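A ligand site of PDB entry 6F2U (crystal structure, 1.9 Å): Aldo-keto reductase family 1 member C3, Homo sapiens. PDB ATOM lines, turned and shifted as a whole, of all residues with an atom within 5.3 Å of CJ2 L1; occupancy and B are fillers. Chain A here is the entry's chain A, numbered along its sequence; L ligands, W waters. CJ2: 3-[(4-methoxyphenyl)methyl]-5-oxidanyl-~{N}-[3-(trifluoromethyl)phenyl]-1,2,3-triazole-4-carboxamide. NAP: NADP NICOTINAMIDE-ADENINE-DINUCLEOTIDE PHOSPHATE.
The side-chain hydroxyl (OH) of Tyr 50 lies within hydrogen-bond range of an oxygen (O15) of CJ2 L1, at 2.6 Å. An oxygen (O15) of CJ2 L1 lies within hydrogen-bond range of a ring nitrogen (NE2) of His 112 (2.7 Å). The backbone NH of Ser 212 sits at hydrogen-bond distance from an oxygen (O5D) of NAP L2, 3.3 Å away. OG of Ser 212 is in hydrogen-bond range of O2N of NAP L2 (2.7 Å). ND2 of Asn 162 lies within hydrogen-bond range of O7N of NAP L2. N of Ser 216 is in hydrogen-bond range of O2A of NAP L2, at 3.0 Å. N of Tyr 19 is in hydrogen-bond range of O3D of NAP L2 (3.1 Å).
N18 of CJ2 L1 sits at hydrogen-bond distance from O7N of NAP L2 (2.7 Å).
The side-chain hydroxyl of Tyr 50 lies within hydrogen-bond range of the side-chain amino group of Lys 79 (2.9 Å). The backbone carbonyl oxygen of His 112 sits at hydrogen-bond distance from the side-chain amide nitrogen of Asn 162 (3.0 Å). The side-chain amide oxygen (OD1) of Asn 162 is in hydrogen-bond range of the side-chain hydroxyl (OH) of Tyr 211. OE2 of Glu 187 sits at hydrogen-bond distance from N of Tyr 300 (2.8 Å). OG of Ser 113 lies within hydrogen-bond range of N of Met 115, at 3.1 Å.
OD1 of Asn 162 sits close to F27 of CJ2 L1. CG of Tyr 19 touches N05 of CJ2 L1, 3.9 Å away. Leu 49 touches CJ2 L1 (CD2 to O17, 3.6 Å). CH2 of Trp 81 touches C22 of CJ2 L1 (3.7 Å). OG of Ser 113 touches C24 of CJ2 L1, at 3.8 Å. OE1 of Glu 187 touches O13 of CJ2 L1, 3.7 Å away. Tyr 211 touches CJ2 L1. Ser 212 touches CJ2 L1 (OG to C14, 3.2 Å). Ser 216 touches CJ2 L1 (CB to C14, 3.9 Å). CZ3 of Trp 222 touches C06 of CJ2 L1, at 3.7 Å. Tyr 300 touches CJ2 L1 (CB to C14, 3.8 Å). Phe 301 touches CJ2 L1 (CE2 to F28, 3.0 Å). Pro 313 touches CJ2 L1 (CG to F26, 3.9 Å). 15 residues have an atom within 4 Å of CJ2 L1: Tyr 19, Leu 49, Tyr 50, Trp 81, His 112, Ser 113, Asn 162, Glu 187, Tyr 211, Ser 212, Ser 216, Trp 222, Tyr 300, Phe 301 and Pro 313.
Water W1 bridges an oxygen (O1N) of NAP L2 (2.8 Å) and a nitrogen (N05) of CJ2 L1 (2.8 Å).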
ATOM      1  N   TYR A  19     -19.038  11.555 -30.136  1.00  0.00           N
ATOM      2  CA  TYR A  19     -17.578  11.499 -30.165  1.00  0.00           C
ATOM      3  C   TYR A  19     -17.084  10.454 -31.168  1.00  0.00           C
ATOM      4  O   TYR A  19     -17.565   9.310 -31.181  1.00  0.00           O
ATOM      5  CB  TYR A  19     -16.971  11.217 -28.797  1.00  0.00           C
ATOM      6  CG  TYR A  19     -15.452  11.168 -28.913  1.00  0.00           C
ATOM      7  CD1 TYR A  19     -14.783   9.959 -28.992  1.00  0.00           C
ATOM      8  CD2 TYR A  19     -14.707  12.346 -29.029  1.00  0.00           C
ATOM      9  CE1 TYR A  19     -13.394   9.922 -29.156  1.00  0.00           C
ATOM     10  CE2 TYR A  19     -13.320  12.316 -29.177  1.00  0.00           C
ATOM     11  CZ  TYR A  19     -12.674  11.094 -29.240  1.00  0.00           C
ATOM     12  OH  TYR A  19     -11.299  11.048 -29.408  1.00  0.00           O
ATOM     13  N   LEU A  49     -14.382  19.393 -26.046  1.00  0.00           N
ATOM     14  CA  LEU A  49     -13.331  18.386 -26.237  1.00  0.00           C
ATOM     15  C   LEU A  49     -13.452  17.643 -27.572  1.00  0.00           C
ATOM     16  O   LEU A  49     -12.430  17.190 -28.117  1.00  0.00           O
ATOM     17  CB  LEU A  49     -13.373  17.374 -25.099  1.00  0.00           C
ATOM     18  CG  LEU A  49     -12.307  16.259 -25.063  1.00  0.00           C
ATOM     19  CD1 LEU A  49     -10.970  16.849 -24.654  1.00  0.00           C
ATOM     20  CD2 LEU A  49     -12.726  15.145 -24.098  1.00  0.00           C
ATOM     21  N   TYR A  50     -14.660  17.437 -28.070  1.00  0.00           N
ATOM     22  CA  TYR A  50     -14.811  16.507 -29.187  1.00  0.00           C
ATOM     23  C   TYR A  50     -14.358  17.083 -30.520  1.00  0.00           C
ATOM     24  O   TYR A  50     -14.235  16.321 -31.484  1.00  0.00           O
ATOM     25  CB  TYR A  50     -16.264  16.036 -29.330  1.00  0.00           C
ATOM     26  CG  TYR A  50     -16.832  15.386 -28.076  1.00  0.00           C
ATOM     27  CD1 TYR A  50     -16.032  15.087 -26.987  1.00  0.00           C
ATOM     28  CD2 TYR A  50     -18.188  15.083 -28.000  1.00  0.00           C
ATOM     29  CE1 TYR A  50     -16.559  14.497 -25.831  1.00  0.00           C
ATOM     30  CE2 TYR A  50     -18.727  14.497 -26.859  1.00  0.00           C
ATOM     31  CZ  TYR A  50     -17.912  14.220 -25.779  1.00  0.00           C
ATOM     32  OH  TYR A  50     -18.449  13.636 -24.652  1.00  0.00           O
ATOM     33  N   LYS A  79     -20.381  20.850 -23.151  1.00  0.00           N
ATOM     34  CA  LYS A  79     -19.659  20.631 -21.902  1.00  0.00           C
ATOM     35  C   LYS A  79     -18.499  21.619 -21.772  1.00  0.00           C
ATOM     36  O   LYS A  79     -17.803  21.885 -22.757  1.00  0.00           O
ATOM     37  CB  LYS A  79     -19.122  19.186 -21.820  1.00  0.00           C
ATOM     38  CG  LYS A  79     -20.202  18.111 -22.075  1.00  0.00           C
ATOM     39  CD  LYS A  79     -19.735  16.702 -21.717  1.00  0.00           C
ATOM     40  CE  LYS A  79     -20.742  15.620 -22.191  1.00  0.00           C
ATOM     41  NZ  LYS A  79     -20.557  15.289 -23.662  1.00  0.00           N
ATOM     42  N   TRP A  81     -14.897  22.459 -20.751  1.00  0.00           N
ATOM     43  CA  TRP A  81     -13.691  21.653 -20.593  1.00  0.00           C
ATOM     44  C   TRP A  81     -12.899  22.123 -19.369  1.00  0.00           C
ATOM     45  O   TRP A  81     -13.099  23.232 -18.843  1.00  0.00           O
ATOM     46  CB  TRP A  81     -12.831  21.661 -21.874  1.00  0.00           C
ATOM     47  CG  TRP A  81     -11.578  20.794 -21.767  1.00  0.00           C
ATOM     48  CD1 TRP A  81     -10.279  21.171 -21.950  1.00  0.00           C
ATOM     49  CD2 TRP A  81     -11.535  19.404 -21.373  1.00  0.00           C
ATOM     50  NE1 TRP A  81      -9.430  20.111 -21.725  1.00  0.00           N
ATOM     51  CE2 TRP A  81     -10.169  19.016 -21.372  1.00  0.00           C
ATOM     52  CE3 TRP A  81     -12.513  18.453 -21.054  1.00  0.00           C
ATOM     53  CZ2 TRP A  81      -9.760  17.725 -21.033  1.00  0.00           C
ATOM     54  CZ3 TRP A  81     -12.097  17.162 -20.721  1.00  0.00           C
ATOM     55  CH2 TRP A  81     -10.736  16.816 -20.720  1.00  0.00           C
ATOM     56  N   HIS A 112     -17.532  19.149 -17.465  1.00  0.00           N
ATOM     57  CA  HIS A 112     -17.193  17.894 -18.136  1.00  0.00           C
ATOM     58  C   HIS A 112     -16.593  16.886 -17.158  1.00  0.00           C
ATOM     59  O   HIS A 112     -16.837  15.687 -17.272  1.00  0.00           O
ATOM     60  CB  HIS A 112     -16.217  18.150 -19.288  1.00  0.00           C
ATOM     61  CG  HIS A 112     -16.178  17.053 -20.309  1.00  0.00           C
ATOM     62  ND1 HIS A 112     -15.992  17.289 -21.655  1.00  0.00           N
ATOM     63  CD2 HIS A 112     -16.289  15.702 -20.185  1.00  0.00           C
ATOM     64  CE1 HIS A 112     -15.993  16.149 -22.312  1.00  0.00           C
ATOM     65  NE2 HIS A 112     -16.176  15.165 -21.445  1.00  0.00           N
ATOM     66  N   SER A 113     -15.802  17.359 -16.194  1.00  0.00           N
ATOM     67  CA  SER A 113     -15.021  16.502 -15.317  1.00  0.00           C
ATOM     68  C   SER A 113     -14.684  17.277 -14.059  1.00  0.00           C
ATOM     69  O   SER A 113     -14.497  18.504 -14.127  1.00  0.00           O
ATOM     70  CB  SER A 113     -13.734  16.036 -16.017  1.00  0.00           C
ATOM     71  OG  SER A 113     -12.736  15.700 -15.058  1.00  0.00           O
ATOM     72  N   PRO A 114     -14.602  16.625 -12.891  1.00  0.00           N
ATOM     73  CA  PRO A 114     -14.242  17.346 -11.664  1.00  0.00           C
ATOM     74  C   PRO A 114     -12.761  17.710 -11.553  1.00  0.00           C
ATOM     75  O   PRO A 114     -12.375  18.384 -10.594  1.00  0.00           O
ATOM     76  CB  PRO A 114     -14.630  16.355 -10.553  1.00  0.00           C
ATOM     77  CG  PRO A 114     -14.497  15.015 -11.192  1.00  0.00           C
ATOM     78  CD  PRO A 114     -14.973  15.216 -12.620  1.00  0.00           C
ATOM     79  N   MET A 115     -11.908  17.312 -12.498  1.00  0.00           N
ATOM     80  CA  MET A 115     -10.459  17.466 -12.355  1.00  0.00           C
ATOM     81  C   MET A 115      -9.972  18.709 -13.112  1.00  0.00           C
ATOM     82  O   MET A 115      -9.754  18.671 -14.322  1.00  0.00           O
ATOM     83  CB  MET A 115      -9.756  16.208 -12.840  1.00  0.00           C
ATOM     84  CG  MET A 115      -9.875  15.089 -11.820  1.00  0.00           C
ATOM     85  SD  MET A 115      -9.644  13.447 -12.488  1.00  0.00           S
ATOM     86  CE  MET A 115      -7.980  13.542 -13.058  1.00  0.00           C
ATOM     87  N   ASN A 162     -19.091  12.971 -14.562  1.00  0.00           N
ATOM     88  CA  ASN A 162     -17.965  12.273 -13.933  1.00  0.00           C
ATOM     89  C   ASN A 162     -17.766  12.647 -12.453  1.00  0.00           C
ATOM     90  O   ASN A 162     -16.658  12.533 -11.931  1.00  0.00           O
ATOM     91  CB  ASN A 162     -16.660  12.496 -14.706  1.00  0.00           C
ATOM     92  CG  ASN A 162     -16.675  11.860 -16.067  1.00  0.00           C
ATOM     93  OD1 ASN A 162     -16.832  10.654 -16.202  1.00  0.00           O
ATOM     94  ND2 ASN A 162     -16.493  12.677 -17.113  1.00  0.00           N
ATOM     95  N   GLU A 187     -19.982   6.995 -16.663  1.00  0.00           N
ATOM     96  CA  GLU A 187     -19.903   5.669 -17.268  1.00  0.00           C
ATOM     97  C   GLU A 187     -20.858   4.719 -16.561  1.00  0.00           C
ATOM     98  O   GLU A 187     -20.870   4.636 -15.323  1.00  0.00           O
ATOM     99  CB  GLU A 187     -18.463   5.135 -17.202  1.00  0.00           C
ATOM    100  CG  GLU A 187     -18.332   3.742 -17.786  1.00  0.00           C
ATOM    101  CD  GLU A 187     -16.915   3.168 -17.724  1.00  0.00           C
ATOM    102  OE1 GLU A 187     -15.946   3.919 -17.474  1.00  0.00           O
ATOM    103  OE2 GLU A 187     -16.787   1.944 -17.939  1.00  0.00           O
ATOM    104  N   TYR A 211     -23.073   7.082 -20.064  1.00  0.00           N
ATOM    105  CA  TYR A 211     -22.220   6.987 -21.244  1.00  0.00           C
ATOM    106  C   TYR A 211     -21.458   5.666 -21.228  1.00  0.00           C
ATOM    107  O   TYR A 211     -21.327   5.010 -20.193  1.00  0.00           O
ATOM    108  CB  TYR A 211     -21.253   8.194 -21.367  1.00  0.00           C
ATOM    109  CG  TYR A 211     -20.048   8.274 -20.409  1.00  0.00           C
ATOM    110  CD1 TYR A 211     -19.950   9.320 -19.499  1.00  0.00           C
ATOM    111  CD2 TYR A 211     -19.016   7.351 -20.461  1.00  0.00           C
ATOM    112  CE1 TYR A 211     -18.848   9.431 -18.634  1.00  0.00           C
ATOM    113  CE2 TYR A 211     -17.907   7.453 -19.604  1.00  0.00           C
ATOM    114  CZ  TYR A 211     -17.830   8.489 -18.692  1.00  0.00           C
ATOM    115  OH  TYR A 211     -16.751   8.599 -17.821  1.00  0.00           O
ATOM    116  N   SER A 212     -20.949   5.301 -22.408  1.00  0.00           N
ATOM    117  CA  SER A 212     -20.349   3.999 -22.674  1.00  0.00           C
ATOM    118  C   SER A 212     -21.329   2.871 -22.340  1.00  0.00           C
ATOM    119  O   SER A 212     -20.940   1.788 -21.873  1.00  0.00           O
ATOM    120  CB  SER A 212     -19.018   3.825 -21.928  1.00  0.00           C
ATOM    121  OG  SER A 212     -18.021   4.686 -22.452  1.00  0.00           O
ATOM    122  N   SER A 216     -18.267   1.133 -24.657  1.00  0.00           N
ATOM    123  CA  SER A 216     -17.220   2.029 -25.110  1.00  0.00           C
ATOM    124  C   SER A 216     -16.712   1.644 -26.490  1.00  0.00           C
ATOM    125  O   SER A 216     -17.009   0.561 -27.008  1.00  0.00           O
ATOM    126  CB  SER A 216     -16.042   2.070 -24.112  1.00  0.00           C
ATOM    127  OG  SER A 216     -14.995   1.195 -24.494  1.00  0.00           O
ATOM    128  N   TRP A 222      -7.013   4.633 -24.190  1.00  0.00           N
ATOM    129  CA  TRP A 222      -7.613   4.692 -22.858  1.00  0.00           C
ATOM    130  C   TRP A 222      -8.269   3.412 -22.403  1.00  0.00           C
ATOM    131  O   TRP A 222      -8.603   3.324 -21.217  1.00  0.00           O
ATOM    132  CB  TRP A 222      -8.663   5.813 -22.774  1.00  0.00           C
ATOM    133  CG  TRP A 222      -8.395   6.997 -23.626  1.00  0.00           C
ATOM    134  CD1 TRP A 222      -7.358   7.888 -23.508  1.00  0.00           C
ATOM    135  CD2 TRP A 222      -9.181   7.453 -24.731  1.00  0.00           C
ATOM    136  NE1 TRP A 222      -7.449   8.857 -24.480  1.00  0.00           N
ATOM    137  CE2 TRP A 222      -8.566   8.613 -25.244  1.00  0.00           C
ATOM    138  CE3 TRP A 222     -10.350   6.984 -25.344  1.00  0.00           C
ATOM    139  CZ2 TRP A 222      -9.073   9.307 -26.342  1.00  0.00           C
ATOM    140  CZ3 TRP A 222     -10.851   7.677 -26.435  1.00  0.00           C
ATOM    141  CH2 TRP A 222     -10.211   8.830 -26.917  1.00  0.00           C
ATOM    142  N   VAL A 223      -8.492   2.429 -23.263  1.00  0.00           N
ATOM    143  CA  VAL A 223      -9.188   1.206 -22.881  1.00  0.00           C
ATOM    144  C   VAL A 223      -8.225   0.029 -23.037  1.00  0.00           C
ATOM    145  O   VAL A 223      -7.608  -0.148 -24.094  1.00  0.00           O
ATOM    146  CB  VAL A 223     -10.468   0.986 -23.702  1.00  0.00           C
ATOM    147  CG1 VAL A 223     -11.119  -0.332 -23.313  1.00  0.00           C
ATOM    148  CG2 VAL A 223     -11.444   2.143 -23.501  1.00  0.00           C
ATOM    149  N   TYR A 300     -14.158   0.849 -18.015  1.00  0.00           N
ATOM    150  CA  TYR A 300     -13.273   0.727 -19.161  1.00  0.00           C
ATOM    151  C   TYR A 300     -12.237   1.850 -19.227  1.00  0.00           C
ATOM    152  O   TYR A 300     -11.194   1.673 -19.873  1.00  0.00           O
ATOM    153  CB  TYR A 300     -14.106   0.720 -20.447  1.00  0.00           C
ATOM    154  CG  TYR A 300     -14.884  -0.561 -20.667  1.00  0.00           C
ATOM    155  CD1 TYR A 300     -16.233  -0.656 -20.315  1.00  0.00           C
ATOM    156  CD2 TYR A 300     -14.276  -1.682 -21.215  1.00  0.00           C
ATOM    157  CE1 TYR A 300     -16.953  -1.851 -20.511  1.00  0.00           C
ATOM    158  CE2 TYR A 300     -14.988  -2.876 -21.417  1.00  0.00           C
ATOM    159  CZ  TYR A 300     -16.315  -2.950 -21.066  1.00  0.00           C
ATOM    160  OH  TYR A 300     -16.997  -4.132 -21.277  1.00  0.00           O
ATOM    161  N   PHE A 301     -12.503   2.990 -18.601  1.00  0.00           N
ATOM    162  CA  PHE A 301     -11.604   4.123 -18.710  1.00  0.00           C
ATOM    163  C   PHE A 301     -10.391   3.890 -17.815  1.00  0.00           C
ATOM    164  O   PHE A 301     -10.537   3.761 -16.594  1.00  0.00           O
ATOM    165  CB  PHE A 301     -12.335   5.418 -18.351  1.00  0.00           C
ATOM    166  CG  PHE A 301     -11.524   6.663 -18.599  1.00  0.00           C
ATOM    167  CD1 PHE A 301     -11.012   6.939 -19.865  1.00  0.00           C
ATOM    168  CD2 PHE A 301     -11.293   7.572 -17.580  1.00  0.00           C
ATOM    169  CE1 PHE A 301     -10.269   8.091 -20.103  1.00  0.00           C
ATOM    170  CE2 PHE A 301     -10.550   8.734 -17.816  1.00  0.00           C
ATOM    171  CZ  PHE A 301     -10.039   8.987 -19.072  1.00  0.00           C
ATOM    172  N   SER A 303      -8.297   5.543 -16.179  1.00  0.00           N
ATOM    173  CA  SER A 303      -8.038   6.830 -15.558  1.00  0.00           C
ATOM    174  C   SER A 303      -6.851   6.810 -14.608  1.00  0.00           C
ATOM    175  O   SER A 303      -6.533   7.858 -14.023  1.00  0.00           O
ATOM    176  CB  SER A 303      -9.283   7.291 -14.790  1.00  0.00           C
ATOM    177  OG  SER A 303      -9.577   6.409 -13.719  1.00  0.00           O
ATOM    178  N   PRO A 313     -12.142  11.040  -9.574  1.00  0.00           N
ATOM    179  CA  PRO A 313     -13.475  10.548  -9.179  1.00  0.00           C
ATOM    180  C   PRO A 313     -13.485   9.101  -8.701  1.00  0.00           C
ATOM    181  O   PRO A 313     -14.409   8.715  -7.962  1.00  0.00           O
ATOM    182  CB  PRO A 313     -14.318  10.730 -10.442  1.00  0.00           C
ATOM    183  CG  PRO A 313     -13.322  10.788 -11.575  1.00  0.00           C
ATOM    184  CD  PRO A 313     -12.093  11.427 -11.000  1.00  0.00           C
ATOM    185  N   TYR A 314     -12.515   8.285  -9.072  1.00  0.00           N
ATOM    186  CA  TYR A 314     -12.600   6.861  -8.750  1.00  0.00           C
ATOM    187  C   TYR A 314     -11.797   6.539  -7.499  1.00  0.00           C
ATOM    188  O   TYR A 314     -10.692   6.025  -7.561  1.00  0.00           O
ATOM    189  CB  TYR A 314     -12.135   6.020  -9.946  1.00  0.00           C
ATOM    190  CG  TYR A 314     -13.100   6.062 -11.114  1.00  0.00           C
ATOM    191  CD1 TYR A 314     -14.475   6.017 -10.900  1.00  0.00           C
ATOM    192  CD2 TYR A 314     -12.652   6.155 -12.431  1.00  0.00           C
ATOM    193  CE1 TYR A 314     -15.379   6.058 -11.973  1.00  0.00           C
ATOM    194  CE2 TYR A 314     -13.547   6.208 -13.509  1.00  0.00           C
ATOM    195  CZ  TYR A 314     -14.906   6.155 -13.259  1.00  0.00           C
ATOM    196  OH  TYR A 314     -15.812   6.201 -14.302  1.00  0.00           O
HETATM  197  C10 CJ2 L   1     -14.389   6.268 -22.895  1.00  0.00           C
HETATM  198  C11 CJ2 L   1     -13.886   7.753 -21.080  1.00  0.00           C
HETATM  199  C14 CJ2 L   1     -15.178   4.338 -21.122  1.00  0.00           C
HETATM  200  C16 CJ2 L   1     -13.642  11.874 -22.252  1.00  0.00           C
HETATM  201  C20 CJ2 L   1     -12.525  13.568 -19.911  1.00  0.00           C
HETATM  202  C22 CJ2 L   1     -11.734  13.868 -18.802  1.00  0.00           C
HETATM  203  C23 CJ2 L   1     -12.718  12.026 -17.585  1.00  0.00           C
HETATM  204  C24 CJ2 L   1     -11.840  13.109 -17.648  1.00  0.00           C
HETATM  205  C25 CJ2 L   1     -12.852  11.174 -16.323  1.00  0.00           C
HETATM  206  C01 CJ2 L   1     -15.844  12.029 -23.732  1.00  0.00           C
HETATM  207  C02 CJ2 L   1     -14.553  11.482 -23.401  1.00  0.00           C
HETATM  208  C06 CJ2 L   1     -13.198   9.645 -24.339  1.00  0.00           C
HETATM  209  C07 CJ2 L   1     -13.583   8.509 -23.367  1.00  0.00           C
HETATM  210  C08 CJ2 L   1     -14.029   7.270 -23.810  1.00  0.00           C
HETATM  211  C09 CJ2 L   1     -13.528   8.723 -21.988  1.00  0.00           C
HETATM  212  C12 CJ2 L   1     -14.310   6.504 -21.530  1.00  0.00           C
HETATM  213  C19 CJ2 L   1     -13.389  12.485 -19.847  1.00  0.00           C
HETATM  214  C21 CJ2 L   1     -13.488  11.724 -18.685  1.00  0.00           C
HETATM  215  F26 CJ2 L   1     -13.478  11.878 -15.341  1.00  0.00           F
HETATM  216  F27 CJ2 L   1     -13.606  10.053 -16.580  1.00  0.00           F
HETATM  217  F28 CJ2 L   1     -11.611  10.808 -15.874  1.00  0.00           F
HETATM  218  N03 CJ2 L   1     -16.282  11.349 -24.807  1.00  0.00           N
HETATM  219  N04 CJ2 L   1     -14.351  10.522 -24.303  1.00  0.00           N
HETATM  220  N05 CJ2 L   1     -15.370  10.452 -25.122  1.00  0.00           N
HETATM  221  N18 CJ2 L   1     -14.230  12.127 -20.966  1.00  0.00           N
HETATM  222  O13 CJ2 L   1     -14.673   5.526 -20.581  1.00  0.00           O
HETATM  223  O15 CJ2 L   1     -16.514  13.049 -23.088  1.00  0.00           O
HETATM  224  O17 CJ2 L   1     -12.472  11.949 -22.396  1.00  0.00           O
HETATM  225  PA  NAP L   2     -20.942   3.634 -26.781  1.00  0.00           P
HETATM  226  O1A NAP L   2     -22.182   4.380 -26.846  1.00  0.00           O
HETATM  227  O2A NAP L   2     -20.548   2.826 -25.523  1.00  0.00           O
HETATM  228  O5B NAP L   2     -21.125   2.633 -28.097  1.00  0.00           O
HETATM  229  C5B NAP L   2     -19.814   2.286 -28.435  1.00  0.00           C
HETATM  230  C4B NAP L   2     -19.760   1.457 -29.711  1.00  0.00           C
HETATM  231  O4B NAP L   2     -20.909   0.643 -29.892  1.00  0.00           O
HETATM  232  C3B NAP L   2     -19.663   2.457 -30.896  1.00  0.00           C
HETATM  233  O3B NAP L   2     -18.326   2.614 -31.251  1.00  0.00           O
HETATM  234  C2B NAP L   2     -20.479   1.758 -32.047  1.00  0.00           C
HETATM  235  O2B NAP L   2     -19.716   1.430 -33.125  1.00  0.00           O
HETATM  236  C1B NAP L   2     -21.057   0.461 -31.318  1.00  0.00           C
HETATM  237  N9A NAP L   2     -22.481   0.307 -31.561  1.00  0.00           N
HETATM  238  C8A NAP L   2     -23.464   1.318 -31.543  1.00  0.00           C
HETATM  239  N7A NAP L   2     -24.700   0.829 -31.804  1.00  0.00           N
HETATM  240  C5A NAP L   2     -24.502  -0.555 -31.994  1.00  0.00           C
HETATM  241  C6A NAP L   2     -25.390  -1.593 -32.294  1.00  0.00           C
HETATM  242  N6A NAP L   2     -26.745  -1.356 -32.455  1.00  0.00           N
HETATM  243  N1A NAP L   2     -24.938  -2.897 -32.439  1.00  0.00           N
HETATM  244  C2A NAP L   2     -23.581  -3.063 -32.277  1.00  0.00           C
HETATM  245  N3A NAP L   2     -22.618  -2.156 -31.989  1.00  0.00           N
HETATM  246  C4A NAP L   2     -23.120  -0.881 -31.848  1.00  0.00           C
HETATM  247  O3  NAP L   2     -19.747   4.687 -27.163  1.00  0.00           O
HETATM  248  PN  NAP L   2     -19.107   5.840 -26.215  1.00  0.00           P
HETATM  249  O1N NAP L   2     -18.530   6.852 -27.097  1.00  0.00           O
HETATM  250  O2N NAP L   2     -18.374   5.244 -25.071  1.00  0.00           O
HETATM  251  O5D NAP L   2     -20.389   6.661 -25.311  1.00  0.00           O
HETATM  252  C5D NAP L   2     -21.195   7.302 -26.228  1.00  0.00           C
HETATM  253  C4D NAP L   2     -21.176   8.850 -26.009  1.00  0.00           C
HETATM  254  O4D NAP L   2     -21.153   9.213 -24.610  1.00  0.00           O
HETATM  255  C3D NAP L   2     -19.910   9.467 -26.611  1.00  0.00           C
HETATM  256  O3D NAP L   2     -20.054   9.560 -27.981  1.00  0.00           O
HETATM  257  C2D NAP L   2     -19.968  10.866 -25.916  1.00  0.00           C
HETATM  258  O2D NAP L   2     -20.979  11.626 -26.454  1.00  0.00           O
HETATM  259  C1D NAP L   2     -20.461  10.451 -24.473  1.00  0.00           C
HETATM  260  N1N NAP L   2     -19.300  10.232 -23.546  1.00  0.00           N
HETATM  261  C2N NAP L   2     -19.106  11.118 -22.513  1.00  0.00           C
HETATM  262  C3N NAP L   2     -18.043  10.954 -21.651  1.00  0.00           C
HETATM  263  C7N NAP L   2     -17.860  11.919 -20.553  1.00  0.00           C
HETATM  264  O7N NAP L   2     -16.766  12.015 -19.960  1.00  0.00           O
HETATM  265  N7N NAP L   2     -18.915  12.685 -20.136  1.00  0.00           N
HETATM  266  C4N NAP L   2     -17.155   9.860 -21.805  1.00  0.00           C
HETATM  267  C5N NAP L   2     -17.384   8.977 -22.848  1.00  0.00           C
HETATM  268  C6N NAP L   2     -18.439   9.152 -23.715  1.00  0.00           C
HETATM  269  P2B NAP L   2     -20.139   1.973 -34.732  1.00  0.00           P
HETATM  270  O1X NAP L   2     -19.971   3.490 -34.524  1.00  0.00           O
HETATM  271  O2X NAP L   2     -19.176   1.296 -35.671  1.00  0.00           O
HETATM  272  O3X NAP L   2     -21.620   1.602 -34.713  1.00  0.00           O
HETATM  273  O   HOH W   1     -16.081   8.037 -26.432  1.00  0.00           O
HETATM  274  O   HOH W   2     -15.852   4.971 -25.600  1.00  0.00           O
